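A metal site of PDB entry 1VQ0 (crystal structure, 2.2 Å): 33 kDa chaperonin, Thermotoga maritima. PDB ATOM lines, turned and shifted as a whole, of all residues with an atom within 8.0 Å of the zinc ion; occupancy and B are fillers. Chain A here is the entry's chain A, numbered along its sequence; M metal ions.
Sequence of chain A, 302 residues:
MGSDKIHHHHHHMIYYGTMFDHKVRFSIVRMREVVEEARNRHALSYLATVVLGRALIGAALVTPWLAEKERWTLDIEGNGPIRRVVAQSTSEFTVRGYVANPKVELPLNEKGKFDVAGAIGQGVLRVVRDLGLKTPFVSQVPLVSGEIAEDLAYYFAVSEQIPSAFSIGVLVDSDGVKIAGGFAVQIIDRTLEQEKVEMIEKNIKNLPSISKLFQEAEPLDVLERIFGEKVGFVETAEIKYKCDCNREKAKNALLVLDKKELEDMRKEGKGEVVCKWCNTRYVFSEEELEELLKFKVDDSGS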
ATOM      1  N   ARG A  41     -27.756 -20.150 -26.033  1.00  0.00           N
ATOM      2  CA  ARG A  41     -28.280 -18.805 -25.714  1.00  0.00           C
ATOM      3  C   ARG A  41     -28.908 -18.164 -26.940  1.00  0.00           C
ATOM      4  O   ARG A  41     -30.051 -17.692 -26.926  1.00  0.00           O
ATOM      5  CB  ARG A  41     -27.158 -17.928 -25.140  1.00  0.00           C
ATOM      6  CG  ARG A  41     -26.829 -18.261 -23.684  1.00  0.00           C
ATOM      7  CD  ARG A  41     -25.771 -17.346 -23.103  1.00  0.00           C
ATOM      8  NE  ARG A  41     -25.574 -17.510 -21.657  1.00  0.00           N
ATOM      9  CZ  ARG A  41     -26.423 -17.085 -20.710  1.00  0.00           C
ATOM     10  NH1 ARG A  41     -27.569 -16.482 -21.000  1.00  0.00           N
ATOM     11  NH2 ARG A  41     -26.121 -17.316 -19.448  1.00  0.00           N
ATOM     12  N   HIS A  42     -28.184 -18.241 -28.053  1.00  0.00           N
ATOM     13  CA  HIS A  42     -28.601 -17.659 -29.328  1.00  0.00           C
ATOM     14  C   HIS A  42     -29.388 -18.568 -30.239  1.00  0.00           C
ATOM     15  O   HIS A  42     -29.760 -18.133 -31.304  1.00  0.00           O
ATOM     16  CB  HIS A  42     -27.357 -17.218 -30.090  1.00  0.00           C
ATOM     17  CG  HIS A  42     -26.639 -16.066 -29.481  1.00  0.00           C
ATOM     18  ND1 HIS A  42     -27.221 -14.825 -29.303  1.00  0.00           N
ATOM     19  CD2 HIS A  42     -25.347 -15.946 -29.048  1.00  0.00           C
ATOM     20  CE1 HIS A  42     -26.320 -13.996 -28.796  1.00  0.00           C
ATOM     21  NE2 HIS A  42     -25.180 -14.656 -28.633  1.00  0.00           N
ATOM     22  N   ARG A  96     -17.809 -13.211 -25.119  1.00  0.00           N
ATOM     23  CA  ARG A  96     -19.182 -13.154 -25.537  1.00  0.00           C
ATOM     24  C   ARG A  96     -19.184 -12.774 -27.004  1.00  0.00           C
ATOM     25  O   ARG A  96     -18.183 -12.329 -27.536  1.00  0.00           O
ATOM     26  CB  ARG A  96     -19.984 -12.166 -24.689  1.00  0.00           C
ATOM     27  CG  ARG A  96     -19.430 -10.719 -24.692  1.00  0.00           C
ATOM     28  CD  ARG A  96     -20.315  -9.744 -23.936  1.00  0.00           C
ATOM     29  NE  ARG A  96     -19.834  -8.396 -24.041  1.00  0.00           N
ATOM     30  CZ  ARG A  96     -20.395  -7.322 -23.533  1.00  0.00           C
ATOM     31  NH1 ARG A  96     -21.560  -7.406 -22.880  1.00  0.00           N
ATOM     32  NH2 ARG A  96     -19.807  -6.130 -23.713  1.00  0.00           N
ATOM     33  N   TYR A 241     -18.029 -18.018 -20.908  1.00  0.00           N
ATOM     34  CA  TYR A 241     -18.963 -17.124 -21.547  1.00  0.00           C
ATOM     35  C   TYR A 241     -19.451 -16.158 -20.465  1.00  0.00           C
ATOM     36  O   TYR A 241     -19.913 -16.588 -19.398  1.00  0.00           O
ATOM     37  CB  TYR A 241     -20.146 -17.885 -22.209  1.00  0.00           C
ATOM     38  CG  TYR A 241     -20.811 -17.104 -23.299  1.00  0.00           C
ATOM     39  CD1 TYR A 241     -21.785 -16.178 -23.006  1.00  0.00           C
ATOM     40  CD2 TYR A 241     -20.394 -17.233 -24.610  1.00  0.00           C
ATOM     41  CE1 TYR A 241     -22.356 -15.429 -24.011  1.00  0.00           C
ATOM     42  CE2 TYR A 241     -20.946 -16.489 -25.613  1.00  0.00           C
ATOM     43  CZ  TYR A 241     -21.939 -15.588 -25.310  1.00  0.00           C
ATOM     44  OH  TYR A 241     -22.510 -14.839 -26.315  1.00  0.00           O
ATOM     45  N   LYS A 242     -19.366 -14.856 -20.720  1.00  0.00           N
ATOM     46  CA  LYS A 242     -19.900 -13.904 -19.774  1.00  0.00           C
ATOM     47  C   LYS A 242     -20.315 -12.590 -20.429  1.00  0.00           C
ATOM     48  O   LYS A 242     -19.628 -12.086 -21.270  1.00  0.00           O
ATOM     49  CB  LYS A 242     -18.894 -13.635 -18.651  1.00  0.00           C
ATOM     50  CG  LYS A 242     -19.587 -13.277 -17.334  1.00  0.00           C
ATOM     51  CD  LYS A 242     -18.603 -12.747 -16.306  1.00  0.00           C
ATOM     52  CE  LYS A 242     -19.315 -11.898 -15.254  1.00  0.00           C
ATOM     53  NZ  LYS A 242     -18.704 -12.106 -13.932  1.00  0.00           N
ATOM     54  N   CYS A 243     -21.460 -12.067 -19.974  1.00  0.00           N
ATOM     55  CA  CYS A 243     -21.997 -10.781 -20.360  1.00  0.00           C
ATOM     56  C   CYS A 243     -22.172  -9.900 -19.078  1.00  0.00           C
ATOM     57  O   CYS A 243     -22.206 -10.412 -18.009  1.00  0.00           O
ATOM     58  CB  CYS A 243     -23.331 -10.974 -21.046  1.00  0.00           C
ATOM     59  SG  CYS A 243     -23.887  -9.529 -21.923  1.00  0.00           S
ATOM     60  N   ASP A 244     -22.239  -8.574 -19.254  1.00  0.00           N
ATOM     61  CA  ASP A 244     -22.374  -7.619 -18.174  1.00  0.00           C
ATOM     62  C   ASP A 244     -23.761  -6.962 -18.237  1.00  0.00           C
ATOM     63  O   ASP A 244     -24.027  -6.010 -17.539  1.00  0.00           O
ATOM     64  CB  ASP A 244     -21.268  -6.529 -18.228  1.00  0.00           C
ATOM     65  CG  ASP A 244     -21.396  -5.607 -19.452  1.00  0.00           C
ATOM     66  OD1 ASP A 244     -22.180  -5.924 -20.329  1.00  0.00           O
ATOM     67  OD2 ASP A 244     -20.770  -4.549 -19.626  1.00  0.00           O
ATOM     68  N   CYS A 245     -24.651  -7.436 -19.096  1.00  0.00           N
ATOM     69  CA  CYS A 245     -25.998  -6.889 -19.054  1.00  0.00           C
ATOM     70  C   CYS A 245     -26.691  -7.256 -17.739  1.00  0.00           C
ATOM     71  O   CYS A 245     -26.334  -8.211 -17.049  1.00  0.00           O
ATOM     72  CB  CYS A 245     -26.830  -7.362 -20.228  1.00  0.00           C
ATOM     73  SG  CYS A 245     -27.306  -9.107 -20.151  1.00  0.00           S
ATOM     74  N   ASN A 246     -27.668  -6.430 -17.388  1.00  0.00           N
ATOM     75  CA  ASN A 246     -28.520  -6.628 -16.249  1.00  0.00           C
ATOM     76  C   ASN A 246     -29.750  -5.740 -16.462  1.00  0.00           C
ATOM     77  O   ASN A 246     -29.843  -4.993 -17.455  1.00  0.00           O
ATOM     78  CB  ASN A 246     -27.834  -6.306 -14.920  1.00  0.00           C
ATOM     79  CG  ASN A 246     -27.417  -4.837 -14.811  1.00  0.00           C
ATOM     80  OD1 ASN A 246     -28.136  -3.939 -15.210  1.00  0.00           O
ATOM     81  ND2 ASN A 246     -26.246  -4.617 -14.240  1.00  0.00           N
ATOM     82  N   VAL A 274     -33.745  -7.103 -25.539  1.00  0.00           N
ATOM     83  CA  VAL A 274     -33.013  -8.351 -25.687  1.00  0.00           C
ATOM     84  C   VAL A 274     -31.534  -7.946 -25.859  1.00  0.00           C
ATOM     85  O   VAL A 274     -31.194  -7.196 -26.744  1.00  0.00           O
ATOM     86  CB  VAL A 274     -33.476  -9.133 -26.929  1.00  0.00           C
ATOM     87  CG1 VAL A 274     -32.636 -10.381 -27.103  1.00  0.00           C
ATOM     88  CG2 VAL A 274     -34.942  -9.464 -26.853  1.00  0.00           C
ATOM     89  N   CYS A 275     -30.685  -8.423 -24.980  1.00  0.00           N
ATOM     90  CA  CYS A 275     -29.250  -8.208 -25.052  1.00  0.00           C
ATOM     91  C   CYS A 275     -28.701  -8.968 -26.254  1.00  0.00           C
ATOM     92  O   CYS A 275     -28.919 -10.181 -26.408  1.00  0.00           O
ATOM     93  CB  CYS A 275     -28.568  -8.695 -23.779  1.00  0.00           C
ATOM     94  SG  CYS A 275     -26.787  -8.649 -23.944  1.00  0.00           S
ATOM     95  N   LYS A 276     -28.015  -8.247 -27.122  1.00  0.00           N
ATOM     96  CA  LYS A 276     -27.538  -8.835 -28.378  1.00  0.00           C
ATOM     97  C   LYS A 276     -26.381  -9.805 -28.098  1.00  0.00           C
ATOM     98  O   LYS A 276     -26.129 -10.706 -28.893  1.00  0.00           O
ATOM     99  CB  LYS A 276     -27.101  -7.733 -29.370  1.00  0.00           C
ATOM    100  CG  LYS A 276     -25.799  -6.984 -28.956  1.00  0.00           C
ATOM    101  CD  LYS A 276     -25.482  -5.762 -29.842  1.00  0.00           C
ATOM    102  CE  LYS A 276     -24.204  -5.074 -29.314  1.00  0.00           C
ATOM    103  NZ  LYS A 276     -23.429  -4.313 -30.356  1.00  0.00           N
ATOM    104  N   TRP A 277     -25.676  -9.611 -26.978  1.00  0.00           N
ATOM    105  CA  TRP A 277     -24.525 -10.464 -26.668  1.00  0.00           C
ATOM    106  C   TRP A 277     -24.848 -11.853 -26.093  1.00  0.00           C
ATOM    107  O   TRP A 277     -24.147 -12.851 -26.366  1.00  0.00           O
ATOM    108  CB  TRP A 277     -23.577  -9.763 -25.729  1.00  0.00           C
ATOM    109  CG  TRP A 277     -22.887  -8.518 -26.214  1.00  0.00           C
ATOM    110  CD1 TRP A 277     -23.238  -7.259 -25.875  1.00  0.00           C
ATOM    111  CD2 TRP A 277     -21.711  -8.383 -27.051  1.00  0.00           C
ATOM    112  NE1 TRP A 277     -22.408  -6.347 -26.476  1.00  0.00           N
ATOM    113  CE2 TRP A 277     -21.432  -7.012 -27.165  1.00  0.00           C
ATOM    114  CE3 TRP A 277     -20.880  -9.277 -27.730  1.00  0.00           C
ATOM    115  CZ2 TRP A 277     -20.352  -6.505 -27.903  1.00  0.00           C
ATOM    116  CZ3 TRP A 277     -19.790  -8.792 -28.435  1.00  0.00           C
ATOM    117  CH2 TRP A 277     -19.557  -7.410 -28.566  1.00  0.00           C
ATOM    118  N   CYS A 278     -25.899 -11.931 -25.294  1.00  0.00           N
ATOM    119  CA  CYS A 278     -26.231 -13.191 -24.650  1.00  0.00           C
ATOM    120  C   CYS A 278     -27.713 -13.581 -24.844  1.00  0.00           C
ATOM    121  O   CYS A 278     -28.145 -14.635 -24.351  1.00  0.00           O
ATOM    122  CB  CYS A 278     -25.860 -13.140 -23.158  1.00  0.00           C
ATOM    123  SG  CYS A 278     -26.996 -12.111 -22.237  1.00  0.00           S
ATOM    124  N   ASN A 279     -28.464 -12.761 -25.575  1.00  0.00           N
ATOM    125  CA  ASN A 279     -29.854 -13.067 -25.885  1.00  0.00           C
ATOM    126  C   ASN A 279     -30.744 -13.177 -24.617  1.00  0.00           C
ATOM    127  O   ASN A 279     -31.774 -13.814 -24.631  1.00  0.00           O
ATOM    128  CB  ASN A 279     -29.962 -14.360 -26.696  1.00  0.00           C
ATOM    129  CG  ASN A 279     -31.275 -14.479 -27.466  1.00  0.00           C
ATOM    130  OD1 ASN A 279     -31.932 -13.497 -27.712  1.00  0.00           O
ATOM    131  ND2 ASN A 279     -31.621 -15.679 -27.860  1.00  0.00           N
ATOM    132  N   THR A 280     -30.334 -12.563 -23.519  1.00  0.00           N
ATOM    133  CA  THR A 280     -31.213 -12.350 -22.387  1.00  0.00           C
ATOM    134  C   THR A 280     -32.247 -11.261 -22.722  1.00  0.00           C
ATOM    135  O   THR A 280     -31.890 -10.165 -23.198  1.00  0.00           O
ATOM    136  CB  THR A 280     -30.444 -11.961 -21.154  1.00  0.00           C
ATOM    137  OG1 THR A 280     -29.530 -13.010 -20.849  1.00  0.00           O
ATOM    138  CG2 THR A 280     -31.396 -11.890 -19.919  1.00  0.00           C
ATOM    139  N   ARG A 281     -33.504 -11.608 -22.465  1.00  0.00           N
ATOM    140  CA  ARG A 281     -34.682 -10.773 -22.636  1.00  0.00           C
ATOM    141  C   ARG A 281     -35.138 -10.176 -21.297  1.00  0.00           C
ATOM    142  O   ARG A 281     -35.183 -10.844 -20.288  1.00  0.00           O
ATOM    143  CB  ARG A 281     -35.828 -11.611 -23.195  1.00  0.00           C
ATOM    144  CG  ARG A 281     -37.101 -10.811 -23.548  1.00  0.00           C
ATOM    145  CD  ARG A 281     -38.269 -11.706 -24.126  1.00  0.00           C
ATOM    146  NE  ARG A 281     -37.763 -12.583 -25.173  1.00  0.00           N
ATOM    147  CZ  ARG A 281     -37.578 -12.224 -26.462  1.00  0.00           C
ATOM    148  NH1 ARG A 281     -37.939 -11.018 -26.900  1.00  0.00           N
ATOM    149  NH2 ARG A 281     -37.054 -13.086 -27.326  1.00  0.00           N
ATOM    150  N   TYR A 282     -35.496  -8.903 -21.365  1.00  0.00           N
ATOM    151  CA  TYR A 282     -35.929  -8.105 -20.252  1.00  0.00           C
ATOM    152  C   TYR A 282     -37.296  -7.549 -20.608  1.00  0.00           C
ATOM    153  O   TYR A 282     -37.445  -6.797 -21.568  1.00  0.00           O
ATOM    154  CB  TYR A 282     -34.923  -6.966 -20.039  1.00  0.00           C
ATOM    155  CG  TYR A 282     -33.557  -7.434 -19.589  1.00  0.00           C
ATOM    156  CD1 TYR A 282     -32.575  -7.769 -20.506  1.00  0.00           C
ATOM    157  CD2 TYR A 282     -33.252  -7.559 -18.244  1.00  0.00           C
ATOM    158  CE1 TYR A 282     -31.329  -8.185 -20.076  1.00  0.00           C
ATOM    159  CE2 TYR A 282     -32.028  -7.991 -17.826  1.00  0.00           C
ATOM    160  CZ  TYR A 282     -31.068  -8.318 -18.725  1.00  0.00           C
ATOM    161  OH  TYR A 282     -29.855  -8.736 -18.279  1.00  0.00           O
HETATM  162 ZN    ZN M   1     -26.180  -9.847 -22.088  1.00  0.00          ZN
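The side-chain sulfur (SG) of Cys 275 lies close to the backbone NH (N) of Trp 277 (3.4 Å).
The backbone NH (N) of Cys 275 lies within hydrogen-bond range of the backbone carbonyl oxygen (O) of Thr 280, at 2.8 Å.
The side-chain sulfur of Cys 243 lies close to the guanidinium group of Arg 96 (3.3 Å).
The side-chain sulfur (SG) of Cys 245 lies close to the side-chain hydroxyl (OH) of Tyr 282 (3.2 Å).
The side-chain sulfur (SG) of Cys 278 lies close to the side-chain hydroxyl (OG1) of Thr 280, 3.0 Å away.
Of the 18 residues printed, 4 come within 4 Å of the zinc ion.
Along chain A the residues within 4 Å of the zinc ion span positions 243 to 278.
The zinc ion is bound by SG of Cys 275 (2.3 Å), SG of Cys 243 (2.3 Å), SG of Cys 245 (2.4 Å) and SG of Cys 278 (2.4 Å).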
